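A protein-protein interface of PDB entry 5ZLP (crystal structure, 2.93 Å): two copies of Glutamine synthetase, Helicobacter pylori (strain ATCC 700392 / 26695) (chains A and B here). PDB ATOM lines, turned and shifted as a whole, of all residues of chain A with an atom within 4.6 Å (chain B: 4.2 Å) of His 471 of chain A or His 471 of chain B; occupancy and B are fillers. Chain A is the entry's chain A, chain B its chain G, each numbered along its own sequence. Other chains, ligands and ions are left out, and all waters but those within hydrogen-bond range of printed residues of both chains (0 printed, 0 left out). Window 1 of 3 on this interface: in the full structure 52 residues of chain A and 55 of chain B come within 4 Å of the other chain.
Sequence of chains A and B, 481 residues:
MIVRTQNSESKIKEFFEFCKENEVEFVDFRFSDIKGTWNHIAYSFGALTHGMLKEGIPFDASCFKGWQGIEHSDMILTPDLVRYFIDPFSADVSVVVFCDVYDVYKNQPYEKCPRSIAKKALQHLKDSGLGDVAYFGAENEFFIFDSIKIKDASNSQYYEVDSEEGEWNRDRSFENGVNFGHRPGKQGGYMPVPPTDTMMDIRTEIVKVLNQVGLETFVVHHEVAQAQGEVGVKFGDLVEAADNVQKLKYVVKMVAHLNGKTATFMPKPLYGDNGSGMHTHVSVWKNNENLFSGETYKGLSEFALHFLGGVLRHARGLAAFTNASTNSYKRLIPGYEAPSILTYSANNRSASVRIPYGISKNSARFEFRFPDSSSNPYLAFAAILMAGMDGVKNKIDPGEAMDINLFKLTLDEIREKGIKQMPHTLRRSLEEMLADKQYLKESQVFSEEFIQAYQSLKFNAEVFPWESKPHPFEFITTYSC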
ATOM      1  N   GLN A 157     -32.743  18.144  10.431  1.00  0.00           N
ATOM      2  CA  GLN A 157     -32.262  16.761  10.531  1.00  0.00           C
ATOM      3  C   GLN A 157     -31.823  16.483  11.963  1.00  0.00           C
ATOM      4  O   GLN A 157     -31.212  17.333  12.606  1.00  0.00           O
ATOM      5  CB  GLN A 157     -31.088  16.457   9.585  1.00  0.00           C
ATOM      6  CG  GLN A 157     -31.304  16.806   8.115  1.00  0.00           C
ATOM      7  CD  GLN A 157     -32.517  16.147   7.507  1.00  0.00           C
ATOM      8  OE1 GLN A 157     -33.292  16.800   6.803  1.00  0.00           O
ATOM      9  NE2 GLN A 157     -32.684  14.850   7.749  1.00  0.00           N
ATOM     10  N   TRP A 466     -27.855  11.073   1.136  1.00  0.00           N
ATOM     11  CA  TRP A 466     -26.759  11.730   1.828  1.00  0.00           C
ATOM     12  C   TRP A 466     -26.313  12.993   1.096  1.00  0.00           C
ATOM     13  O   TRP A 466     -26.064  14.035   1.722  1.00  0.00           O
ATOM     14  CB  TRP A 466     -25.605  10.747   1.982  1.00  0.00           C
ATOM     15  CG  TRP A 466     -24.549  11.224   2.910  1.00  0.00           C
ATOM     16  CD1 TRP A 466     -24.718  11.718   4.179  1.00  0.00           C
ATOM     17  CD2 TRP A 466     -23.144  11.238   2.658  1.00  0.00           C
ATOM     18  NE1 TRP A 466     -23.498  12.051   4.722  1.00  0.00           N
ATOM     19  CE2 TRP A 466     -22.517  11.762   3.805  1.00  0.00           C
ATOM     20  CE3 TRP A 466     -22.359  10.869   1.573  1.00  0.00           C
ATOM     21  CZ2 TRP A 466     -21.146  11.913   3.893  1.00  0.00           C
ATOM     22  CZ3 TRP A 466     -21.002  11.018   1.665  1.00  0.00           C
ATOM     23  CH2 TRP A 466     -20.407  11.537   2.812  1.00  0.00           C
ATOM     24  N   LYS A 469     -29.295  15.782   1.532  1.00  0.00           N
ATOM     25  CA  LYS A 469     -29.898  16.167   2.793  1.00  0.00           C
ATOM     26  C   LYS A 469     -28.901  16.970   3.598  1.00  0.00           C
ATOM     27  O   LYS A 469     -27.830  16.446   3.943  1.00  0.00           O
ATOM     28  CB  LYS A 469     -30.365  14.953   3.586  1.00  0.00           C
ATOM     29  CG  LYS A 469     -31.805  14.561   3.308  1.00  0.00           C
ATOM     30  CD  LYS A 469     -32.064  13.170   3.840  1.00  0.00           C
ATOM     31  CE  LYS A 469     -33.287  12.576   3.221  1.00  0.00           C
ATOM     32  NZ  LYS A 469     -34.486  13.317   3.663  1.00  0.00           N
ATOM     33  N   PRO A 470     -29.214  18.229   3.897  1.00  0.00           N
ATOM     34  CA  PRO A 470     -28.334  19.059   4.729  1.00  0.00           C
ATOM     35  C   PRO A 470     -27.902  18.357   6.008  1.00  0.00           C
ATOM     36  O   PRO A 470     -28.721  17.782   6.727  1.00  0.00           O
ATOM     37  CB  PRO A 470     -29.198  20.284   5.027  1.00  0.00           C
ATOM     38  CG  PRO A 470     -30.123  20.355   3.892  1.00  0.00           C
ATOM     39  CD  PRO A 470     -30.386  18.970   3.408  1.00  0.00           C
ATOM     40  N   HIS A 471     -26.562  18.397   6.280  1.00  0.00           N
ATOM     41  CA  HIS A 471     -25.929  17.847   7.477  1.00  0.00           C
ATOM     42  C   HIS A 471     -25.917  18.896   8.594  1.00  0.00           C
ATOM     43  O   HIS A 471     -25.571  20.054   8.338  1.00  0.00           O
ATOM     44  CB  HIS A 471     -24.500  17.372   7.179  1.00  0.00           C
ATOM     45  CG  HIS A 471     -23.893  16.574   8.295  1.00  0.00           C
ATOM     46  ND1 HIS A 471     -23.496  17.145   9.489  1.00  0.00           N
ATOM     47  CD2 HIS A 471     -23.659  15.245   8.421  1.00  0.00           C
ATOM     48  CE1 HIS A 471     -23.038  16.207  10.300  1.00  0.00           C
ATOM     49  NE2 HIS A 471     -23.119  15.045   9.674  1.00  0.00           N
ATOM     50  N   PRO A 472     -26.352  18.559   9.830  1.00  0.00           N
ATOM     51  CA  PRO A 472     -26.196  19.496  10.954  1.00  0.00           C
ATOM     52  C   PRO A 472     -24.932  20.355  10.931  1.00  0.00           C
ATOM     53  O   PRO A 472     -25.032  21.584  11.007  1.00  0.00           O
ATOM     54  CB  PRO A 472     -26.236  18.555  12.162  1.00  0.00           C
ATOM     55  CG  PRO A 472     -27.196  17.438  11.684  1.00  0.00           C
ATOM     56  CD  PRO A 472     -27.329  17.512  10.177  1.00  0.00           C
ATOM     57  N   PHE A 473     -23.755  19.736  10.770  1.00  0.00           N
ATOM     58  CA  PHE A 473     -22.503  20.471  10.922  1.00  0.00           C
ATOM     59  C   PHE A 473     -22.360  21.611   9.913  1.00  0.00           C
ATOM     60  O   PHE A 473     -21.833  22.682  10.246  1.00  0.00           O
ATOM     61  CB  PHE A 473     -21.322  19.528  10.794  1.00  0.00           C
ATOM     62  CG  PHE A 473     -20.030  20.156  11.204  1.00  0.00           C
ATOM     63  CD1 PHE A 473     -19.919  20.793  12.447  1.00  0.00           C
ATOM     64  CD2 PHE A 473     -18.924  20.131  10.363  1.00  0.00           C
ATOM     65  CE1 PHE A 473     -18.721  21.398  12.856  1.00  0.00           C
ATOM     66  CE2 PHE A 473     -17.728  20.732  10.745  1.00  0.00           C
ATOM     67  CZ  PHE A 473     -17.616  21.370  12.004  1.00  0.00           C
ATOM     68  N   GLU A 474     -22.818  21.398   8.675  1.00  0.00           N
ATOM     69  CA  GLU A 474     -22.788  22.445   7.660  1.00  0.00           C
ATOM     70  C   GLU A 474     -23.354  23.751   8.184  1.00  0.00           C
ATOM     71  O   GLU A 474     -23.017  24.821   7.662  1.00  0.00           O
ATOM     72  CB  GLU A 474     -23.578  22.009   6.411  1.00  0.00           C
ATOM     73  CG  GLU A 474     -23.228  20.600   5.920  1.00  0.00           C
ATOM     74  CD  GLU A 474     -23.923  20.187   4.620  1.00  0.00           C
ATOM     75  OE1 GLU A 474     -25.088  20.608   4.366  1.00  0.00           O
ATOM     76  OE2 GLU A 474     -23.280  19.427   3.851  1.00  0.00           O
ATOM     77  N   PHE A 475     -24.226  23.686   9.198  1.00  0.00           N
ATOM     78  CA  PHE A 475     -24.835  24.900   9.736  1.00  0.00           C
ATOM     79  C   PHE A 475     -23.880  25.624  10.658  1.00  0.00           C
ATOM     80  O   PHE A 475     -23.948  26.849  10.778  1.00  0.00           O
ATOM     81  CB  PHE A 475     -26.159  24.565  10.429  1.00  0.00           C
ATOM     82  CG  PHE A 475     -27.263  24.286   9.458  1.00  0.00           C
ATOM     83  CD1 PHE A 475     -27.308  23.088   8.774  1.00  0.00           C
ATOM     84  CD2 PHE A 475     -28.210  25.242   9.176  1.00  0.00           C
ATOM     85  CE1 PHE A 475     -28.302  22.851   7.846  1.00  0.00           C
ATOM     86  CE2 PHE A 475     -29.195  25.011   8.267  1.00  0.00           C
ATOM     87  CZ  PHE A 475     -29.244  23.826   7.593  1.00  0.00           C
ATOM     88  N   GLN B 157     -26.372  14.704  16.286  1.00  0.00           N
ATOM     89  CA  GLN B 157     -26.262  15.801  15.342  1.00  0.00           C
ATOM     90  C   GLN B 157     -27.657  16.341  15.100  1.00  0.00           C
ATOM     91  O   GLN B 157     -28.609  15.566  14.976  1.00  0.00           O
ATOM     92  CB  GLN B 157     -25.626  15.338  14.042  1.00  0.00           C
ATOM     93  CG  GLN B 157     -24.246  14.734  14.230  1.00  0.00           C
ATOM     94  CD  GLN B 157     -23.162  15.768  14.367  1.00  0.00           C
ATOM     95  OE1 GLN B 157     -23.088  16.726  13.593  1.00  0.00           O
ATOM     96  NE2 GLN B 157     -22.309  15.584  15.349  1.00  0.00           N
ATOM     97  N   TRP B 466     -17.580  16.335   7.281  1.00  0.00           N
ATOM     98  CA  TRP B 466     -18.744  15.723   6.654  1.00  0.00           C
ATOM     99  C   TRP B 466     -18.504  14.237   6.353  1.00  0.00           C
ATOM    100  O   TRP B 466     -19.440  13.424   6.436  1.00  0.00           O
ATOM    101  CB  TRP B 466     -19.117  16.532   5.395  1.00  0.00           C
ATOM    102  CG  TRP B 466     -20.358  16.091   4.664  1.00  0.00           C
ATOM    103  CD1 TRP B 466     -21.647  16.148   5.113  1.00  0.00           C
ATOM    104  CD2 TRP B 466     -20.419  15.549   3.335  1.00  0.00           C
ATOM    105  NE1 TRP B 466     -22.503  15.662   4.157  1.00  0.00           N
ATOM    106  CE2 TRP B 466     -21.776  15.279   3.058  1.00  0.00           C
ATOM    107  CE3 TRP B 466     -19.455  15.242   2.364  1.00  0.00           C
ATOM    108  CZ2 TRP B 466     -22.197  14.721   1.847  1.00  0.00           C
ATOM    109  CZ3 TRP B 466     -19.869  14.689   1.171  1.00  0.00           C
ATOM    110  CH2 TRP B 466     -21.232  14.444   0.917  1.00  0.00           C
ATOM    111  N   LYS B 469     -18.832  12.595  10.330  1.00  0.00           N
ATOM    112  CA  LYS B 469     -19.901  12.778  11.305  1.00  0.00           C
ATOM    113  C   LYS B 469     -21.167  12.062  10.849  1.00  0.00           C
ATOM    114  O   LYS B 469     -21.690  12.384   9.778  1.00  0.00           O
ATOM    115  CB  LYS B 469     -20.175  14.263  11.524  1.00  0.00           C
ATOM    116  CG  LYS B 469     -19.107  14.964  12.364  1.00  0.00           C
ATOM    117  CD  LYS B 469     -19.273  16.471  12.406  1.00  0.00           C
ATOM    118  CE  LYS B 469     -18.238  17.115  13.330  1.00  0.00           C
ATOM    119  NZ  LYS B 469     -18.121  16.354  14.618  1.00  0.00           N
ATOM    120  N   PRO B 470     -21.689  11.108  11.625  1.00  0.00           N
ATOM    121  CA  PRO B 470     -22.933  10.420  11.246  1.00  0.00           C
ATOM    122  C   PRO B 470     -24.063  11.395  10.956  1.00  0.00           C
ATOM    123  O   PRO B 470     -24.232  12.409  11.641  1.00  0.00           O
ATOM    124  CB  PRO B 470     -23.257   9.566  12.477  1.00  0.00           C
ATOM    125  CG  PRO B 470     -22.014   9.494  13.264  1.00  0.00           C
ATOM    126  CD  PRO B 470     -21.225  10.725  12.969  1.00  0.00           C
ATOM    127  N   HIS B 471     -24.844  11.072   9.932  1.00  0.00           N
ATOM    128  CA  HIS B 471     -25.954  11.867   9.449  1.00  0.00           C
ATOM    129  C   HIS B 471     -27.247  11.299   9.979  1.00  0.00           C
ATOM    130  O   HIS B 471     -27.408  10.081  10.007  1.00  0.00           O
ATOM    131  CB  HIS B 471     -26.005  11.879   7.923  1.00  0.00           C
ATOM    132  CG  HIS B 471     -26.952  12.894   7.359  1.00  0.00           C
ATOM    133  ND1 HIS B 471     -28.313  12.685   7.285  1.00  0.00           N
ATOM    134  CD2 HIS B 471     -26.733  14.134   6.853  1.00  0.00           C
ATOM    135  CE1 HIS B 471     -28.888  13.749   6.748  1.00  0.00           C
ATOM    136  NE2 HIS B 471     -27.953  14.641   6.476  1.00  0.00           N
ATOM    137  N   PRO B 472     -28.165  12.155  10.439  1.00  0.00           N
ATOM    138  CA  PRO B 472     -29.429  11.650  10.988  1.00  0.00           C
ATOM    139  C   PRO B 472     -30.069  10.582  10.119  1.00  0.00           C
ATOM    140  O   PRO B 472     -30.454   9.521  10.628  1.00  0.00           O
ATOM    141  CB  PRO B 472     -30.279  12.917  11.078  1.00  0.00           C
ATOM    142  CG  PRO B 472     -29.264  13.950  11.474  1.00  0.00           C
ATOM    143  CD  PRO B 472     -27.983  13.584  10.748  1.00  0.00           C
ATOM    144  N   PHE B 473     -30.113  10.819   8.803  1.00  0.00           N
ATOM    145  CA  PHE B 473     -30.824   9.912   7.907  1.00  0.00           C
ATOM    146  C   PHE B 473     -30.199   8.517   7.859  1.00  0.00           C
ATOM    147  O   PHE B 473     -30.883   7.557   7.472  1.00  0.00           O
ATOM    148  CB  PHE B 473     -30.890  10.512   6.508  1.00  0.00           C
ATOM    149  CG  PHE B 473     -31.753   9.733   5.571  1.00  0.00           C
ATOM    150  CD1 PHE B 473     -33.145   9.900   5.595  1.00  0.00           C
ATOM    151  CD2 PHE B 473     -31.184   8.816   4.679  1.00  0.00           C
ATOM    152  CE1 PHE B 473     -33.961   9.189   4.750  1.00  0.00           C
ATOM    153  CE2 PHE B 473     -31.981   8.091   3.836  1.00  0.00           C
ATOM    154  CZ  PHE B 473     -33.390   8.283   3.868  1.00  0.00           C
ATOM    155  N   GLU B 474     -28.924   8.385   8.257  1.00  0.00           N
ATOM    156  CA  GLU B 474     -28.262   7.090   8.341  1.00  0.00           C
ATOM    157  C   GLU B 474     -28.804   6.235   9.483  1.00  0.00           C
ATOM    158  O   GLU B 474     -28.669   5.005   9.442  1.00  0.00           O
ATOM    159  CB  GLU B 474     -26.756   7.290   8.503  1.00  0.00           C
ATOM    160  CG  GLU B 474     -26.191   8.291   7.539  1.00  0.00           C
ATOM    161  CD  GLU B 474     -24.677   8.306   7.459  1.00  0.00           C
ATOM    162  OE1 GLU B 474     -24.171   8.579   6.356  1.00  0.00           O
ATOM    163  OE2 GLU B 474     -23.990   8.073   8.469  1.00  0.00           O
ATOM    164  N   PHE B 475     -29.412   6.847  10.495  1.00  0.00           N
ATOM    165  CA  PHE B 475     -30.085   6.052  11.510  1.00  0.00           C
ATOM    166  C   PHE B 475     -31.455   5.593  11.049  1.00  0.00           C
ATOM    167  O   PHE B 475     -31.984   4.613  11.579  1.00  0.00           O
ATOM    168  CB  PHE B 475     -30.201   6.838  12.806  1.00  0.00           C
ATOM    169  CG  PHE B 475     -28.877   7.179  13.408  1.00  0.00           C
ATOM    170  CD1 PHE B 475     -28.069   8.150  12.832  1.00  0.00           C
ATOM    171  CD2 PHE B 475     -28.423   6.523  14.538  1.00  0.00           C
ATOM    172  CE1 PHE B 475     -26.850   8.450  13.366  1.00  0.00           C
ATOM    173  CE2 PHE B 475     -27.206   6.827  15.077  1.00  0.00           C
ATOM    174  CZ  PHE B 475     -26.415   7.776  14.487  1.00  0.00           C
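The backbone carbonyl oxygen (O) of Lys 469 of chain A is in hydrogen-bond range of a ring nitrogen (NE2) of His 471 of chain B (3.1 Å).
A ring nitrogen (NE2) of His 471 of chain B is in hydrogen-bond range of the backbone carbonyl oxygen of Pro 470 of chain A (3.2 Å).
O of Pro 470 of chain B sits at hydrogen-bond distance from NE2 of His 471 of chain A, 3.5 Å away.
O of Lys 469 of chain B sits at hydrogen-bond distance from NE2 of His 471 of chain A (3.0 Å).
Gln 157 of chain A touches Gln 157 of chain B.
CB of Gln 157 of chain A touches CG of Pro 472 of chain B (3.6 Å).
Trp 466 of chain A touches Trp 466 of chain B (CZ2 to O, 3.4 Å).
Trp 466 of chain A touches His 471 of chain B.
CD1 of Trp 466 of chain A touches OE1 of Glu 474 of chain B (3.9 Å).
CD1 of Phe 473 of chain B touches CE of Lys 469 of chain A (3.6 Å).
OE1 of Gln 157 of chain B touches CE1 of His 471 of chain A, 3.3 Å away.
His 471 of chain A touches Trp 466 of chain B.
His 471 of chain A touches His 471 of chain B (CD2 to CD2, 3.6 Å).
CD of Lys 469 of chain B touches CG of Phe 473 of chain A (3.9 Å).
N of Phe 473 of chain A sits at hydrogen-bond distance from ND1 of His 471 of chain A.
The side-chain carboxylate (OE2) of Glu 474 of chain B lies within hydrogen-bond range of the backbone NH (N) of His 471 of chain B (3.4 Å).
N of Phe 473 of chain B sits at hydrogen-bond distance from ND1 of His 471 of chain B (3.0 Å).
The side-chain carboxylate of Glu 474 of chain A is in hydrogen-bond range of the backbone NH of His 471 of chain A (3.3 Å).
Among the printed residues, 16 pairs touch across the chains.
His 471 of chain A touches just these residues of chain B: Gln 157, Trp 466, Lys 469, Pro 470 and His 471.
Of the printed residues of chain B, Pro 472 of chain A touches Gln 157.
Of the printed residues of chain A, Lys 469 of chain B touches His 471 and Phe 473.
Of chain A, only Trp 466, Lys 469, Pro 470 and His 471 come within 4 Å of His 471 of chain B.
Of the printed residues of chain A, Phe 473 of chain B touches Lys 469.
Printed residues of chain A within 4 Å of Glu 474 of chain B: Trp 466 (3.9 Å).
The nearest residue of chain A that does not touch His 471 of chain B is Gln 157 of chain A (4.1 Å).
The nearest printed residue of chain A that does not touch Glu 474 of chain B is His 471 of chain A (7.0 Å).
Gln 157 of chain A touches Pro 472 of chain B, and with the chains exchanged Pro 472 of chain A touches Gln 157 of chain B.
Trp 466 of chain A touches His 471 of chain B, and with the chains exchanged His 471 of chain A touches Trp 466 of chain B.
Trp 466 of chain A touches Glu 474 of chain B, and with the chains exchanged Glu 474 of chain A touches Trp 466 of chain B.
Lys 469 of chain A touches Phe 473 of chain B, and with the chains exchanged Phe 473 of chain A touches Lys 469 of chain B.
9 positions are printed for both chains.
Of the 16 pairs that touch across the chains among the printed residues, 15 have their exchanged pair printed and touching as well.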
